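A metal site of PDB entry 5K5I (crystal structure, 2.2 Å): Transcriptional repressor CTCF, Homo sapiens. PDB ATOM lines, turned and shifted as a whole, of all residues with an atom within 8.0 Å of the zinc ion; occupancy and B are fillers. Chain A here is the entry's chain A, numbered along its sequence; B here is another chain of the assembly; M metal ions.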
ATOM      1  N   GLN A   8      10.651  -3.513   9.086  1.00  0.00           N
ATOM      2  CA  GLN A   8      11.468  -2.570   9.843  1.00  0.00           C
ATOM      3  C   GLN A   8      12.940  -2.977   9.753  1.00  0.00           C
ATOM      4  O   GLN A   8      13.275  -4.154   9.866  1.00  0.00           O
ATOM      5  CB  GLN A   8      11.037  -2.508  11.303  1.00  0.00           C
ATOM      6  CG  GLN A   8      11.795  -1.500  12.156  1.00  0.00           C
ATOM      7  CD  GLN A   8      11.452  -0.068  11.802  1.00  0.00           C
ATOM      8  OE1 GLN A   8      10.321   0.247  11.456  1.00  0.00           O
ATOM      9  NE2 GLN A   8      12.447   0.808  11.894  1.00  0.00           N
ATOM     10  N   CYS A   9      13.805  -1.983   9.560  1.00  0.00           N
ATOM     11  CA  CYS A   9      15.244  -2.242   9.529  1.00  0.00           C
ATOM     12  C   CYS A   9      15.764  -2.512  10.934  1.00  0.00           C
ATOM     13  O   CYS A   9      15.256  -1.990  11.931  1.00  0.00           O
ATOM     14  CB  CYS A   9      15.983  -1.064   8.900  1.00  0.00           C
ATOM     15  SG  CYS A   9      17.779  -1.289   8.813  1.00  0.00           S
ATOM     16  N   SER A  10      16.820  -3.338  11.008  1.00  0.00           N
ATOM     17  CA  SER A  10      17.363  -3.742  12.295  1.00  0.00           C
ATOM     18  C   SER A  10      18.369  -2.733  12.841  1.00  0.00           C
ATOM     19  O   SER A  10      18.461  -2.555  14.050  1.00  0.00           O
ATOM     20  CB  SER A  10      18.013  -5.115  12.180  1.00  0.00           C
ATOM     21  OG  SER A  10      17.099  -6.081  11.702  1.00  0.00           O
ATOM     22  N   LEU A  11      19.129  -2.080  11.962  1.00  0.00           N
ATOM     23  CA  LEU A  11      20.216  -1.200  12.383  1.00  0.00           C
ATOM     24  C   LEU A  11      19.863   0.276  12.331  1.00  0.00           C
ATOM     25  O   LEU A  11      20.670   1.101  12.772  1.00  0.00           O
ATOM     26  CB  LEU A  11      21.466  -1.456  11.532  1.00  0.00           C
ATOM     27  CG  LEU A  11      22.001  -2.893  11.555  1.00  0.00           C
ATOM     28  CD1 LEU A  11      23.271  -3.005  10.733  1.00  0.00           C
ATOM     29  CD2 LEU A  11      22.220  -3.361  12.980  1.00  0.00           C
ATOM     30  N   CYS A  12      18.689   0.639  11.826  1.00  0.00           N
ATOM     31  CA  CYS A  12      18.281   2.037  11.775  1.00  0.00           C
ATOM     32  C   CYS A  12      16.762   2.098  11.803  1.00  0.00           C
ATOM     33  O   CYS A  12      16.077   1.092  12.038  1.00  0.00           O
ATOM     34  CB  CYS A  12      18.865   2.736  10.539  1.00  0.00           C
ATOM     35  SG  CYS A  12      18.008   2.379   8.990  1.00  0.00           S
ATOM     36  N   SER A  13      16.216   3.296  11.560  1.00  0.00           N
ATOM     37  CA  SER A  13      14.784   3.545  11.670  1.00  0.00           C
ATOM     38  C   SER A  13      14.039   3.423  10.345  1.00  0.00           C
ATOM     39  O   SER A  13      12.836   3.698  10.301  1.00  0.00           O
ATOM     40  CB  SER A  13      14.546   4.935  12.265  1.00  0.00           C
ATOM     41  OG  SER A  13      15.198   5.068  13.514  1.00  0.00           O
ATOM     42  N   TYR A  14      14.726   3.031   9.268  1.00  0.00           N
ATOM     43  CA  TYR A  14      14.064   2.946   7.969  1.00  0.00           C
ATOM     44  C   TYR A  14      13.051   1.802   7.953  1.00  0.00           C
ATOM     45  O   TYR A  14      13.293   0.730   8.499  1.00  0.00           O
ATOM     46  CB  TYR A  14      15.093   2.746   6.863  1.00  0.00           C
ATOM     47  CG  TYR A  14      14.481   2.594   5.490  1.00  0.00           C
ATOM     48  CD1 TYR A  14      14.065   3.705   4.762  1.00  0.00           C
ATOM     49  CD2 TYR A  14      14.314   1.341   4.916  1.00  0.00           C
ATOM     50  CE1 TYR A  14      13.499   3.571   3.510  1.00  0.00           C
ATOM     51  CE2 TYR A  14      13.746   1.193   3.661  1.00  0.00           C
ATOM     52  CZ  TYR A  14      13.345   2.317   2.964  1.00  0.00           C
ATOM     53  OH  TYR A  14      12.785   2.176   1.710  1.00  0.00           O
ATOM     54  N   ALA A  15      11.921   2.052   7.312  1.00  0.00           N
ATOM     55  CA  ALA A  15      10.870   1.048   7.179  1.00  0.00           C
ATOM     56  C   ALA A  15      10.186   1.220   5.829  1.00  0.00           C
ATOM     57  O   ALA A  15      10.142   2.324   5.270  1.00  0.00           O
ATOM     58  CB  ALA A  15       9.841   1.162   8.316  1.00  0.00           C
ATOM     59  N   LEU A  22      13.591  -2.837   1.438  1.00  0.00           N
ATOM     60  CA  LEU A  22      14.450  -3.060   2.594  1.00  0.00           C
ATOM     61  C   LEU A  22      15.720  -3.817   2.205  1.00  0.00           C
ATOM     62  O   LEU A  22      16.804  -3.520   2.720  1.00  0.00           O
ATOM     63  CB  LEU A  22      13.693  -3.810   3.688  1.00  0.00           C
ATOM     64  CG  LEU A  22      14.492  -4.175   4.945  1.00  0.00           C
ATOM     65  CD1 LEU A  22      14.981  -2.928   5.656  1.00  0.00           C
ATOM     66  CD2 LEU A  22      13.696  -5.055   5.891  1.00  0.00           C
ATOM     67  N   HIS A  25      17.832  -1.195   0.910  1.00  0.00           N
ATOM     68  CA  HIS A  25      18.311  -0.318   1.973  1.00  0.00           C
ATOM     69  C   HIS A  25      19.416  -0.967   2.796  1.00  0.00           C
ATOM     70  O   HIS A  25      20.302  -0.271   3.298  1.00  0.00           O
ATOM     71  CB  HIS A  25      17.146   0.111   2.872  1.00  0.00           C
ATOM     72  CG  HIS A  25      17.589   0.743   4.164  1.00  0.00           C
ATOM     73  ND1 HIS A  25      18.140   2.000   4.224  1.00  0.00           N
ATOM     74  CD2 HIS A  25      17.561   0.279   5.431  1.00  0.00           C
ATOM     75  CE1 HIS A  25      18.424   2.287   5.482  1.00  0.00           C
ATOM     76  NE2 HIS A  25      18.089   1.264   6.241  1.00  0.00           N
ATOM     77  N   MET A  26      19.367  -2.295   2.954  1.00  0.00           N
ATOM     78  CA  MET A  26      20.371  -2.974   3.765  1.00  0.00           C
ATOM     79  C   MET A  26      21.771  -2.877   3.169  1.00  0.00           C
ATOM     80  O   MET A  26      22.758  -3.067   3.898  1.00  0.00           O
ATOM     81  CB  MET A  26      19.992  -4.442   3.941  1.00  0.00           C
ATOM     82  CG  MET A  26      18.862  -4.683   4.929  1.00  0.00           C
ATOM     83  SD  MET A  26      19.218  -3.971   6.554  1.00  0.00           S
ATOM     84  CE  MET A  26      17.979  -4.782   7.562  1.00  0.00           C
ATOM     85  N   ARG A  27      21.887  -2.570   1.873  1.00  0.00           N
ATOM     86  CA  ARG A  27      23.209  -2.397   1.265  1.00  0.00           C
ATOM     87  C   ARG A  27      23.948  -1.188   1.826  1.00  0.00           C
ATOM     88  O   ARG A  27      25.178  -1.136   1.754  1.00  0.00           O
ATOM     89  CB  ARG A  27      23.062  -2.269  -0.249  1.00  0.00           C
ATOM     90  CG  ARG A  27      22.340  -3.433  -0.905  1.00  0.00           C
ATOM     91  CD  ARG A  27      22.064  -3.159  -2.367  1.00  0.00           C
ATOM     92  NE  ARG A  27      21.207  -4.186  -2.960  1.00  0.00           N
ATOM     93  CZ  ARG A  27      20.678  -4.113  -4.181  1.00  0.00           C
ATOM     94  NH1 ARG A  27      20.915  -3.056  -4.948  1.00  0.00           N
ATOM     95  NH2 ARG A  27      19.912  -5.097  -4.633  1.00  0.00           N
ATOM     96  N   THR A  28      23.222  -0.215   2.389  1.00  0.00           N
ATOM     97  CA  THR A  28      23.880   0.935   2.989  1.00  0.00           C
ATOM     98  C   THR A  28      24.654   0.553   4.246  1.00  0.00           C
ATOM     99  O   THR A  28      25.703   1.144   4.533  1.00  0.00           O
ATOM    100  CB  THR A  28      22.844   2.019   3.324  1.00  0.00           C
ATOM    101  OG1 THR A  28      21.944   1.542   4.327  1.00  0.00           O
ATOM    102  CG2 THR A  28      22.056   2.387   2.077  1.00  0.00           C
ATOM    103  N   HIS A  29      24.162  -0.439   4.995  1.00  0.00           N
ATOM    104  CA  HIS A  29      24.831  -0.915   6.194  1.00  0.00           C
ATOM    105  C   HIS A  29      25.893  -1.966   5.894  1.00  0.00           C
ATOM    106  O   HIS A  29      27.000  -1.908   6.444  1.00  0.00           O
ATOM    107  CB  HIS A  29      23.809  -1.496   7.171  1.00  0.00           C
ATOM    108  CG  HIS A  29      22.755  -0.527   7.617  1.00  0.00           C
ATOM    109  ND1 HIS A  29      23.034   0.548   8.424  1.00  0.00           N
ATOM    110  CD2 HIS A  29      21.430  -0.474   7.365  1.00  0.00           C
ATOM    111  CE1 HIS A  29      21.926   1.235   8.648  1.00  0.00           C
ATOM    112  NE2 HIS A  29      20.934   0.622   8.015  1.00  0.00           N
ATOM    113  P    DA B   9      18.541   4.290   1.454  1.00  0.00           P
ATOM    114  OP1  DA B   9      18.465   4.182   2.924  1.00  0.00           O
ATOM    115  OP2  DA B   9      18.846   3.086   0.642  1.00  0.00           O
ATOM    116  O5'  DA B   9      17.165   4.900   0.923  1.00  0.00           O
ATOM    117  C5'  DA B   9      16.741   6.175   1.385  1.00  0.00           C
ATOM    118  C4'  DA B   9      15.573   6.689   0.561  1.00  0.00           C
ATOM    119  O4'  DA B   9      15.979   6.815  -0.831  1.00  0.00           O
ATOM    120  C3'  DA B   9      14.332   5.793   0.575  1.00  0.00           C
ATOM    121  O3'  DA B   9      13.165   6.599   0.700  1.00  0.00           O
ATOM    122  C2'  DA B   9      14.392   5.096  -0.778  1.00  0.00           C
ATOM    123  C1'  DA B   9      15.031   6.160  -1.657  1.00  0.00           C
ATOM    124  N9   DA B   9      15.746   5.608  -2.806  1.00  0.00           N
ATOM    125  C8   DA B   9      16.650   4.584  -2.806  1.00  0.00           C
ATOM    126  N7   DA B   9      17.120   4.307  -4.000  1.00  0.00           N
ATOM    127  C5   DA B   9      16.478   5.203  -4.837  1.00  0.00           C
ATOM    128  C6   DA B   9      16.542   5.412  -6.220  1.00  0.00           C
ATOM    129  N6   DA B   9      17.330   4.700  -7.044  1.00  0.00           N
ATOM    130  N1   DA B   9      15.773   6.394  -6.748  1.00  0.00           N
ATOM    131  C2   DA B   9      14.990   7.098  -5.927  1.00  0.00           C
ATOM    132  N3   DA B   9      14.843   6.989  -4.602  1.00  0.00           N
ATOM    133  C4   DA B   9      15.625   6.006  -4.117  1.00  0.00           C
HETATM  134 ZN    ZN M   1      18.911   0.565   7.968  1.00  0.00          ZN
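The zinc ion is bound by NE2 of His 29 (2.0 Å), NE2 of His 25 (2.0 Å), SG of Cys 12 (2.3 Å) and SG of Cys 9 of chain A (2.3 Å).
The zinc ion has four donor atoms within binding distance.
Four residues have an atom within 4 Å of the zinc ion: Cys 9 of chain A, Cys 12, His 25 and His 29.
The nearest printed residue that does not touch the zinc ion is Leu 11 (4.5 Å).
The backbone carbonyl oxygen of His 25 is in hydrogen-bond range of the side-chain hydroxyl of Thr 28, at 2.7 Å.
A ring nitrogen (ND1) of His 25 is in hydrogen-bond range of OP1 of DA 9 of chain B, at 2.6 Å.
The backbone NH (N) of Tyr 14 sits close to the side-chain sulfur (SG) of Cys 12 (3.4 Å).
The side-chain sulfur (SG) of Cys 9 of chain A lies close to the backbone NH (N) of Leu 11.
N of Cys 9 of chain A is in hydrogen-bond range of O of Tyr 14.
The side-chain sulfur (SG) of Cys 9 of chain A lies close to the side-chain sulfur (SD) of Met 26, at 3.8 Å.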
